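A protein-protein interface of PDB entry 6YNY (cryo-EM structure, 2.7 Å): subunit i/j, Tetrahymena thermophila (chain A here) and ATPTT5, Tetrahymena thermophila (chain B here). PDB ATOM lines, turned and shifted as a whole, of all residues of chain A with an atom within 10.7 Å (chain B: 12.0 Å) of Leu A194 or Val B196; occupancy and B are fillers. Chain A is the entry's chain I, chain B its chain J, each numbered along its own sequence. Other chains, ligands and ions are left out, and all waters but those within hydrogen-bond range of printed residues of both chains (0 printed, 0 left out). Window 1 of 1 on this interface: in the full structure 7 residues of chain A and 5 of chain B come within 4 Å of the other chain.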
ATOM      1  N   THR A 176      -8.517 -21.287  -4.821  1.00  0.00           N
ATOM      2  CA  THR A 176      -7.423 -21.172  -5.769  1.00  0.00           C
ATOM      3  C   THR A 176      -7.832 -20.300  -6.948  1.00  0.00           C
ATOM      4  O   THR A 176      -9.012 -20.197  -7.292  1.00  0.00           O
ATOM      5  CB  THR A 176      -7.003 -22.553  -6.265  1.00  0.00           C
ATOM      6  OG1 THR A 176      -6.824 -23.428  -5.146  1.00  0.00           O
ATOM      7  CG2 THR A 176      -5.706 -22.469  -7.049  1.00  0.00           C
ATOM      8  N   ASP A 177      -6.833 -19.667  -7.570  1.00  0.00           N
ATOM      9  CA  ASP A 177      -7.099 -18.832  -8.735  1.00  0.00           C
ATOM     10  C   ASP A 177      -7.849 -19.600  -9.812  1.00  0.00           C
ATOM     11  O   ASP A 177      -8.672 -19.025 -10.532  1.00  0.00           O
ATOM     12  CB  ASP A 177      -5.785 -18.289  -9.292  1.00  0.00           C
ATOM     13  CG  ASP A 177      -5.994 -17.241 -10.364  1.00  0.00           C
ATOM     14  OD1 ASP A 177      -6.370 -16.102 -10.014  1.00  0.00           O
ATOM     15  OD2 ASP A 177      -5.779 -17.552 -11.554  1.00  0.00           O
ATOM     16  N   GLN A 178      -7.582 -20.901  -9.935  1.00  0.00           N
ATOM     17  CA  GLN A 178      -8.280 -21.714 -10.924  1.00  0.00           C
ATOM     18  C   GLN A 178      -9.757 -21.853 -10.581  1.00  0.00           C
ATOM     19  O   GLN A 178     -10.613 -21.812 -11.471  1.00  0.00           O
ATOM     20  CB  GLN A 178      -7.612 -23.086 -11.020  1.00  0.00           C
ATOM     21  CG  GLN A 178      -8.415 -24.158 -11.739  1.00  0.00           C
ATOM     22  CD  GLN A 178      -8.731 -23.800 -13.172  1.00  0.00           C
ATOM     23  OE1 GLN A 178      -9.132 -22.678 -13.470  1.00  0.00           O
ATOM     24  NE2 GLN A 178      -8.551 -24.756 -14.072  1.00  0.00           N
ATOM     25  N   LYS A 180     -11.691 -19.800  -8.652  1.00  0.00           N
ATOM     26  CA  LYS A 180     -12.412 -18.537  -8.693  1.00  0.00           C
ATOM     27  C   LYS A 180     -12.509 -17.948 -10.092  1.00  0.00           C
ATOM     28  O   LYS A 180     -13.173 -16.921 -10.266  1.00  0.00           O
ATOM     29  CB  LYS A 180     -11.751 -17.526  -7.756  1.00  0.00           C
ATOM     30  CG  LYS A 180     -10.320 -17.211  -8.093  1.00  0.00           C
ATOM     31  CD  LYS A 180      -9.769 -16.118  -7.197  1.00  0.00           C
ATOM     32  CE  LYS A 180      -9.701 -16.560  -5.754  1.00  0.00           C
ATOM     33  NZ  LYS A 180      -8.955 -15.592  -4.917  1.00  0.00           N
ATOM     34  N   LYS A 181     -11.869 -18.558 -11.088  1.00  0.00           N
ATOM     35  CA  LYS A 181     -11.976 -18.103 -12.463  1.00  0.00           C
ATOM     36  C   LYS A 181     -12.729 -19.069 -13.364  1.00  0.00           C
ATOM     37  O   LYS A 181     -13.009 -18.718 -14.515  1.00  0.00           O
ATOM     38  CB  LYS A 181     -10.581 -17.852 -13.050  1.00  0.00           C
ATOM     39  CG  LYS A 181      -9.879 -16.653 -12.458  1.00  0.00           C
ATOM     40  CD  LYS A 181      -8.749 -16.173 -13.341  1.00  0.00           C
ATOM     41  CE  LYS A 181      -8.014 -15.007 -12.720  1.00  0.00           C
ATOM     42  NZ  LYS A 181      -8.935 -13.902 -12.353  1.00  0.00           N
ATOM     43  N   TYR A 189     -15.262 -21.057 -21.894  1.00  0.00           N
ATOM     44  CA  TYR A 189     -14.036 -20.414 -21.444  1.00  0.00           C
ATOM     45  C   TYR A 189     -12.994 -21.463 -21.088  1.00  0.00           C
ATOM     46  O   TYR A 189     -13.270 -22.388 -20.318  1.00  0.00           O
ATOM     47  CB  TYR A 189     -14.310 -19.515 -20.239  1.00  0.00           C
ATOM     48  CG  TYR A 189     -13.062 -18.972 -19.587  1.00  0.00           C
ATOM     49  CD1 TYR A 189     -12.294 -18.008 -20.217  1.00  0.00           C
ATOM     50  CD2 TYR A 189     -12.659 -19.414 -18.338  1.00  0.00           C
ATOM     51  CE1 TYR A 189     -11.159 -17.507 -19.625  1.00  0.00           C
ATOM     52  CE2 TYR A 189     -11.524 -18.919 -17.741  1.00  0.00           C
ATOM     53  CZ  TYR A 189     -10.778 -17.963 -18.390  1.00  0.00           C
ATOM     54  OH  TYR A 189      -9.642 -17.457 -17.807  1.00  0.00           O
ATOM     55  N   GLN A 190     -11.799 -21.312 -21.650  1.00  0.00           N
ATOM     56  CA  GLN A 190     -10.661 -22.159 -21.326  1.00  0.00           C
ATOM     57  C   GLN A 190      -9.734 -21.394 -20.393  1.00  0.00           C
ATOM     58  O   GLN A 190      -9.246 -20.315 -20.743  1.00  0.00           O
ATOM     59  CB  GLN A 190      -9.913 -22.583 -22.590  1.00  0.00           C
ATOM     60  CG  GLN A 190     -10.653 -23.591 -23.449  1.00  0.00           C
ATOM     61  CD  GLN A 190     -11.881 -23.006 -24.109  1.00  0.00           C
ATOM     62  OE1 GLN A 190     -12.101 -21.797 -24.074  1.00  0.00           O
ATOM     63  NE2 GLN A 190     -12.689 -23.863 -24.720  1.00  0.00           N
ATOM     64  N   TYR A 191      -9.496 -21.952 -19.211  1.00  0.00           N
ATOM     65  CA  TYR A 191      -8.683 -21.272 -18.214  1.00  0.00           C
ATOM     66  C   TYR A 191      -7.219 -21.272 -18.629  1.00  0.00           C
ATOM     67  O   TYR A 191      -6.669 -22.306 -19.019  1.00  0.00           O
ATOM     68  CB  TYR A 191      -8.851 -21.938 -16.853  1.00  0.00           C
ATOM     69  CG  TYR A 191      -7.908 -21.414 -15.797  1.00  0.00           C
ATOM     70  CD1 TYR A 191      -8.045 -20.132 -15.291  1.00  0.00           C
ATOM     71  CD2 TYR A 191      -6.890 -22.209 -15.295  1.00  0.00           C
ATOM     72  CE1 TYR A 191      -7.189 -19.654 -14.324  1.00  0.00           C
ATOM     73  CE2 TYR A 191      -6.031 -21.739 -14.326  1.00  0.00           C
ATOM     74  CZ  TYR A 191      -6.185 -20.461 -13.844  1.00  0.00           C
ATOM     75  OH  TYR A 191      -5.331 -19.987 -12.878  1.00  0.00           O
ATOM     76  N   SER A 192      -6.593 -20.104 -18.545  1.00  0.00           N
ATOM     77  CA  SER A 192      -5.169 -19.944 -18.827  1.00  0.00           C
ATOM     78  C   SER A 192      -4.553 -19.140 -17.691  1.00  0.00           C
ATOM     79  O   SER A 192      -4.896 -17.951 -17.525  1.00  0.00           O
ATOM     80  CB  SER A 192      -4.952 -19.255 -20.171  1.00  0.00           C
ATOM     81  OG  SER A 192      -5.726 -18.074 -20.264  1.00  0.00           O
ATOM     82  N   PRO A 193      -3.663 -19.727 -16.890  1.00  0.00           N
ATOM     83  CA  PRO A 193      -3.150 -19.015 -15.716  1.00  0.00           C
ATOM     84  C   PRO A 193      -2.521 -17.678 -16.073  1.00  0.00           C
ATOM     85  O   PRO A 193      -1.967 -17.490 -17.157  1.00  0.00           O
ATOM     86  CB  PRO A 193      -2.111 -19.982 -15.144  1.00  0.00           C
ATOM     87  CG  PRO A 193      -2.543 -21.314 -15.606  1.00  0.00           C
ATOM     88  CD  PRO A 193      -3.154 -21.107 -16.953  1.00  0.00           C
ATOM     89  N   LEU A 194      -2.618 -16.746 -15.136  1.00  0.00           N
ATOM     90  CA  LEU A 194      -1.993 -15.440 -15.223  1.00  0.00           C
ATOM     91  C   LEU A 194      -0.811 -15.350 -14.268  1.00  0.00           C
ATOM     92  O   LEU A 194      -0.746 -16.077 -13.272  1.00  0.00           O
ATOM     93  CB  LEU A 194      -2.999 -14.334 -14.885  1.00  0.00           C
ATOM     94  CG  LEU A 194      -3.927 -13.881 -16.008  1.00  0.00           C
ATOM     95  CD1 LEU A 194      -5.173 -13.254 -15.437  1.00  0.00           C
ATOM     96  CD2 LEU A 194      -3.216 -12.893 -16.905  1.00  0.00           C
ATOM     97  N   PRO A 195       0.147 -14.468 -14.542  1.00  0.00           N
ATOM     98  CA  PRO A 195       1.261 -14.289 -13.607  1.00  0.00           C
ATOM     99  C   PRO A 195       0.770 -13.881 -12.227  1.00  0.00           C
ATOM    100  O   PRO A 195      -0.140 -13.061 -12.086  1.00  0.00           O
ATOM    101  CB  PRO A 195       2.097 -13.184 -14.258  1.00  0.00           C
ATOM    102  CG  PRO A 195       1.748 -13.239 -15.692  1.00  0.00           C
ATOM    103  CD  PRO A 195       0.323 -13.669 -15.765  1.00  0.00           C
ATOM    104  N   VAL A 196       1.389 -14.465 -11.203  1.00  0.00           N
ATOM    105  CA  VAL A 196       0.997 -14.185  -9.829  1.00  0.00           C
ATOM    106  C   VAL A 196       1.474 -12.794  -9.438  1.00  0.00           C
ATOM    107  O   VAL A 196       2.620 -12.414  -9.705  1.00  0.00           O
ATOM    108  CB  VAL A 196       1.560 -15.256  -8.884  1.00  0.00           C
ATOM    109  CG1 VAL A 196       1.152 -14.969  -7.454  1.00  0.00           C
ATOM    110  CG2 VAL A 196       1.083 -16.627  -9.305  1.00  0.00           C
ATOM    111  N   VAL A 197       0.587 -12.026  -8.804  1.00  0.00           N
ATOM    112  CA  VAL A 197       0.902 -10.685  -8.333  1.00  0.00           C
ATOM    113  C   VAL A 197       0.336 -10.518  -6.931  1.00  0.00           C
ATOM    114  O   VAL A 197      -0.531 -11.274  -6.490  1.00  0.00           O
ATOM    115  CB  VAL A 197       0.350  -9.587  -9.266  1.00  0.00           C
ATOM    116  CG1 VAL A 197       1.061  -9.626 -10.601  1.00  0.00           C
ATOM    117  CG2 VAL A 197      -1.143  -9.756  -9.458  1.00  0.00           C
ATOM    118  N   SER A 198       0.837  -9.504  -6.233  1.00  0.00           N
ATOM    119  CA  SER A 198       0.418  -9.215  -4.866  1.00  0.00           C
ATOM    120  C   SER A 198      -0.758  -8.248  -4.902  1.00  0.00           C
ATOM    121  O   SER A 198      -0.589  -7.060  -5.193  1.00  0.00           O
ATOM    122  CB  SER A 198       1.575  -8.634  -4.059  1.00  0.00           C
ATOM    123  OG  SER A 198       2.657  -9.546  -3.984  1.00  0.00           O
ATOM    124  N   ILE A 199      -1.949  -8.759  -4.607  1.00  0.00           N
ATOM    125  CA  ILE A 199      -3.157  -7.943  -4.554  1.00  0.00           C
ATOM    126  C   ILE A 199      -3.842  -8.217  -3.220  1.00  0.00           C
ATOM    127  O   ILE A 199      -4.419  -9.297  -3.035  1.00  0.00           O
ATOM    128  CB  ILE A 199      -4.085  -8.241  -5.738  1.00  0.00           C
ATOM    129  CG1 ILE A 199      -3.388  -7.878  -7.047  1.00  0.00           C
ATOM    130  CG2 ILE A 199      -5.374  -7.466  -5.601  1.00  0.00           C
ATOM    131  CD1 ILE A 199      -4.112  -8.338  -8.274  1.00  0.00           C
ATOM    132  N   MET B 185     -13.157  -6.496 -28.123  1.00  0.00           N
ATOM    133  CA  MET B 185     -12.557  -7.812 -28.265  1.00  0.00           C
ATOM    134  C   MET B 185     -11.756  -7.958 -29.547  1.00  0.00           C
ATOM    135  O   MET B 185     -11.309  -9.064 -29.861  1.00  0.00           O
ATOM    136  CB  MET B 185     -13.643  -8.884 -28.206  1.00  0.00           C
ATOM    137  CG  MET B 185     -14.450  -8.854 -26.928  1.00  0.00           C
ATOM    138  SD  MET B 185     -13.463  -9.163 -25.458  1.00  0.00           S
ATOM    139  CE  MET B 185     -13.036 -10.875 -25.721  1.00  0.00           C
ATOM    140  N   VAL B 187      -8.550  -7.833 -31.838  1.00  0.00           N
ATOM    141  CA  VAL B 187      -7.126  -8.019 -31.596  1.00  0.00           C
ATOM    142  C   VAL B 187      -6.360  -7.077 -32.513  1.00  0.00           C
ATOM    143  O   VAL B 187      -6.422  -7.204 -33.740  1.00  0.00           O
ATOM    144  CB  VAL B 187      -6.710  -9.478 -31.826  1.00  0.00           C
ATOM    145  CG1 VAL B 187      -5.245  -9.661 -31.513  1.00  0.00           C
ATOM    146  CG2 VAL B 187      -7.554 -10.401 -30.971  1.00  0.00           C
ATOM    147  N   TYR B 190      -0.625  -4.843 -32.600  1.00  0.00           N
ATOM    148  CA  TYR B 190       0.407  -4.897 -31.574  1.00  0.00           C
ATOM    149  C   TYR B 190       0.157  -5.977 -30.531  1.00  0.00           C
ATOM    150  O   TYR B 190       0.959  -6.117 -29.603  1.00  0.00           O
ATOM    151  CB  TYR B 190       0.541  -3.535 -30.882  1.00  0.00           C
ATOM    152  CG  TYR B 190      -0.750  -2.956 -30.353  1.00  0.00           C
ATOM    153  CD1 TYR B 190      -1.282  -3.382 -29.148  1.00  0.00           C
ATOM    154  CD2 TYR B 190      -1.426  -1.971 -31.053  1.00  0.00           C
ATOM    155  CE1 TYR B 190      -2.457  -2.854 -28.661  1.00  0.00           C
ATOM    156  CE2 TYR B 190      -2.601  -1.435 -30.574  1.00  0.00           C
ATOM    157  CZ  TYR B 190      -3.111  -1.881 -29.376  1.00  0.00           C
ATOM    158  OH  TYR B 190      -4.283  -1.354 -28.888  1.00  0.00           O
ATOM    159  N   ASN B 191      -0.928  -6.745 -30.658  1.00  0.00           N
ATOM    160  CA  ASN B 191      -1.217  -7.836 -29.734  1.00  0.00           C
ATOM    161  C   ASN B 191      -1.507  -9.142 -30.464  1.00  0.00           C
ATOM    162  O   ASN B 191      -2.100 -10.054 -29.879  1.00  0.00           O
ATOM    163  CB  ASN B 191      -2.386  -7.474 -28.816  1.00  0.00           C
ATOM    164  CG  ASN B 191      -1.933  -6.848 -27.517  1.00  0.00           C
ATOM    165  OD1 ASN B 191      -0.783  -6.995 -27.109  1.00  0.00           O
ATOM    166  ND2 ASN B 191      -2.845  -6.158 -26.849  1.00  0.00           N
ATOM    167  N   GLN B 192      -1.099  -9.260 -31.724  1.00  0.00           N
ATOM    168  CA  GLN B 192      -1.305 -10.499 -32.459  1.00  0.00           C
ATOM    169  C   GLN B 192      -0.456 -11.612 -31.861  1.00  0.00           C
ATOM    170  O   GLN B 192       0.754 -11.453 -31.673  1.00  0.00           O
ATOM    171  CB  GLN B 192      -0.956 -10.306 -33.932  1.00  0.00           C
ATOM    172  CG  GLN B 192      -1.854  -9.330 -34.665  1.00  0.00           C
ATOM    173  CD  GLN B 192      -3.266  -9.850 -34.843  1.00  0.00           C
ATOM    174  OE1 GLN B 192      -3.573 -10.984 -34.478  1.00  0.00           O
ATOM    175  NE2 GLN B 192      -4.135  -9.020 -35.409  1.00  0.00           N
ATOM    176  N   GLY B 193      -1.093 -12.739 -31.559  1.00  0.00           N
ATOM    177  CA  GLY B 193      -0.387 -13.890 -31.039  1.00  0.00           C
ATOM    178  C   GLY B 193      -0.007 -13.810 -29.580  1.00  0.00           C
ATOM    179  O   GLY B 193       0.701 -14.698 -29.094  1.00  0.00           O
ATOM    180  N   ARG B 194      -0.450 -12.783 -28.866  1.00  0.00           N
ATOM    181  CA  ARG B 194      -0.136 -12.617 -27.456  1.00  0.00           C
ATOM    182  C   ARG B 194      -1.297 -13.103 -26.601  1.00  0.00           C
ATOM    183  O   ARG B 194      -2.464 -12.856 -26.919  1.00  0.00           O
ATOM    184  CB  ARG B 194       0.171 -11.154 -27.143  1.00  0.00           C
ATOM    185  CG  ARG B 194       1.565 -10.722 -27.553  1.00  0.00           C
ATOM    186  CD  ARG B 194       1.745  -9.221 -27.470  1.00  0.00           C
ATOM    187  NE  ARG B 194       1.347  -8.677 -26.176  1.00  0.00           N
ATOM    188  CZ  ARG B 194       2.147  -8.594 -25.119  1.00  0.00           C
ATOM    189  NH1 ARG B 194       1.690  -8.083 -23.988  1.00  0.00           N
ATOM    190  NH2 ARG B 194       3.399  -9.021 -25.185  1.00  0.00           N
ATOM    191  N   THR B 195      -0.966 -13.800 -25.514  1.00  0.00           N
ATOM    192  CA  THR B 195      -1.973 -14.347 -24.615  1.00  0.00           C
ATOM    193  C   THR B 195      -1.694 -13.920 -23.180  1.00  0.00           C
ATOM    194  O   THR B 195      -0.813 -13.093 -22.933  1.00  0.00           O
ATOM    195  CB  THR B 195      -2.006 -15.872 -24.710  1.00  0.00           C
ATOM    196  OG1 THR B 195      -0.729 -16.405 -24.339  1.00  0.00           O
ATOM    197  CG2 THR B 195      -2.340 -16.310 -26.124  1.00  0.00           C
ATOM    198  N   VAL B 196      -2.442 -14.481 -22.228  1.00  0.00           N
ATOM    199  CA  VAL B 196      -2.243 -14.138 -20.827  1.00  0.00           C
ATOM    200  C   VAL B 196      -0.852 -14.526 -20.356  1.00  0.00           C
ATOM    201  O   VAL B 196      -0.347 -13.960 -19.383  1.00  0.00           O
ATOM    202  CB  VAL B 196      -3.318 -14.813 -19.950  1.00  0.00           C
ATOM    203  CG1 VAL B 196      -4.701 -14.392 -20.387  1.00  0.00           C
ATOM    204  CG2 VAL B 196      -3.184 -16.317 -20.000  1.00  0.00           C
ATOM    205  N   ALA B 197      -0.219 -15.488 -21.026  1.00  0.00           N
ATOM    206  CA  ALA B 197       1.121 -15.906 -20.632  1.00  0.00           C
ATOM    207  C   ALA B 197       2.156 -14.825 -20.904  1.00  0.00           C
ATOM    208  O   ALA B 197       3.152 -14.727 -20.180  1.00  0.00           O
ATOM    209  CB  ALA B 197       1.494 -17.192 -21.363  1.00  0.00           C
ATOM    210  N   ASP B 198       1.942 -14.007 -21.930  1.00  0.00           N
ATOM    211  CA  ASP B 198       2.862 -12.931 -22.266  1.00  0.00           C
ATOM    212  C   ASP B 198       2.619 -11.668 -21.453  1.00  0.00           C
ATOM    213  O   ASP B 198       3.240 -10.638 -21.737  1.00  0.00           O
ATOM    214  CB  ASP B 198       2.760 -12.608 -23.757  1.00  0.00           C
ATOM    215  CG  ASP B 198       3.041 -13.809 -24.633  1.00  0.00           C
ATOM    216  OD1 ASP B 198       3.820 -14.686 -24.207  1.00  0.00           O
ATOM    217  OD2 ASP B 198       2.482 -13.878 -25.747  1.00  0.00           O
ATOM    218  N   VAL B 199       1.745 -11.717 -20.467  1.00  0.00           N
ATOM    219  CA  VAL B 199       1.452 -10.564 -19.627  1.00  0.00           C
ATOM    220  C   VAL B 199       2.468 -10.498 -18.499  1.00  0.00           C
ATOM    221  O   VAL B 199       2.979 -11.521 -18.031  1.00  0.00           O
ATOM    222  CB  VAL B 199       0.010 -10.632 -19.088  1.00  0.00           C
ATOM    223  CG1 VAL B 199      -0.254  -9.496 -18.136  1.00  0.00           C
ATOM    224  CG2 VAL B 199      -0.974 -10.591 -20.229  1.00  0.00           C
ATOM    225  N   ALA B 200       2.768  -9.285 -18.060  1.00  0.00           N
ATOM    226  CA  ALA B 200       3.750  -9.084 -17.010  1.00  0.00           C
ATOM    227  C   ALA B 200       3.098  -9.138 -15.633  1.00  0.00           C
ATOM    228  O   ALA B 200       1.917  -8.807 -15.483  1.00  0.00           O
ATOM    229  CB  ALA B 200       4.443  -7.741 -17.186  1.00  0.00           C
ATOM    230  N   PRO B 201       3.844  -9.548 -14.607  1.00  0.00           N
ATOM    231  CA  PRO B 201       3.299  -9.578 -13.235  1.00  0.00           C
ATOM    232  C   PRO B 201       3.335  -8.200 -12.584  1.00  0.00           C
ATOM    233  O   PRO B 201       4.054  -7.937 -11.614  1.00  0.00           O
ATOM    234  CB  PRO B 201       4.216 -10.588 -12.544  1.00  0.00           C
ATOM    235  CG  PRO B 201       5.520 -10.408 -13.224  1.00  0.00           C
ATOM    236  CD  PRO B 201       5.216 -10.079 -14.659  1.00  0.00           C
ATOM    237  N   LYS B 202       2.536  -7.289 -13.130  1.00  0.00           N
ATOM    238  CA  LYS B 202       2.504  -5.907 -12.687  1.00  0.00           C
ATOM    239  C   LYS B 202       1.078  -5.522 -12.323  1.00  0.00           C
ATOM    240  O   LYS B 202       0.110  -6.117 -12.803  1.00  0.00           O
ATOM    241  CB  LYS B 202       3.047  -4.973 -13.773  1.00  0.00           C
ATOM    242  CG  LYS B 202       4.414  -5.379 -14.292  1.00  0.00           C
ATOM    243  CD  LYS B 202       4.812  -4.592 -15.526  1.00  0.00           C
ATOM    244  CE  LYS B 202       5.235  -3.182 -15.194  1.00  0.00           C
ATOM    245  NZ  LYS B 202       6.500  -3.157 -14.421  1.00  0.00           N
ATOM    246  N   THR B 203       0.961  -4.521 -11.460  1.00  0.00           N
ATOM    247  CA  THR B 203      -0.321  -4.000 -11.011  1.00  0.00           C
ATOM    248  C   THR B 203      -0.423  -2.521 -11.364  1.00  0.00           C
ATOM    249  O   THR B 203       0.451  -1.951 -12.018  1.00  0.00           O
ATOM    250  CB  THR B 203      -0.506  -4.215  -9.510  1.00  0.00           C
ATOM    251  OG1 THR B 203       0.566  -3.593  -8.795  1.00  0.00           O
ATOM    252  CG2 THR B 203      -0.531  -5.686  -9.194  1.00  0.00           C
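Val B196 touches Ser A192. CG2 of Val B196 touches O of Pro A193 (3.3 Å). Val B196 touches Leu A194 (CB to CD2, 3.6 Å). CD of Pro A195 touches O of Val B196, 3.7 Å away. Pro A195 touches Val B199 (CG to O, 3.2 Å). Pro A195 touches Pro B201 (CB to CB, 3.8 Å). Pro B201 touches Val A196. CG1 of Val A197 touches C of Pro B201, at 3.3 Å. Val A197 touches Lys B202. Val A197 touches Thr B203 (CB to CG2, 3.9999 Å).
Gln A190 touches none of the printed residues of chain B. Ser A192 touches just one residue of chain B: Val B196 (3.1 Å). Pro A193 touches just one residue of chain B: Val B196. Leu A194 touches just one residue of chain B: Val B196. Pro A195 touches three residues of chain B. Val A196 touches just one residue of chain B: Pro B201. Printed residues of chain B within 4 Å of Val A197: Pro B201 (3.3 Å), Lys B202 (3.7 Å) and Thr B203 (3.9999 Å). Of chain A, only Ser A192, Pro A193, Leu A194 and Pro A195 come within 4 Å of Val B196. Val B199 touches just one residue of chain A: Pro A195 (3.2 Å). Of the printed residues of chain A, Pro B201 touches Pro A195 (3.8 Å), Val A196 (3.7 Å) and Val A197 (3.3 Å). Of the printed residues of chain A, Thr B203 touches Val A197 (3.9999 Å). The nearest residue of chain B that does not touch Leu A194 is Val B199 (4.5 Å).
Of the 16 printed residues of chain B, 5 touch a printed residue of chain A. Printed residues of chain B that touch a printed residue of chain A: Val B196, Val B199, Pro B201, Lys B202 and Thr B203. Hydrophobic or aromatic side chains of chain B that line the printed part of chain A: Val B196 and Pro B201. Among the printed residues, 10 pairs touch across the chains. Among the printed residues, no Asp or Glu carboxylate lies within 4 Å of a Lys or Arg side-chain nitrogen of the other chain.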
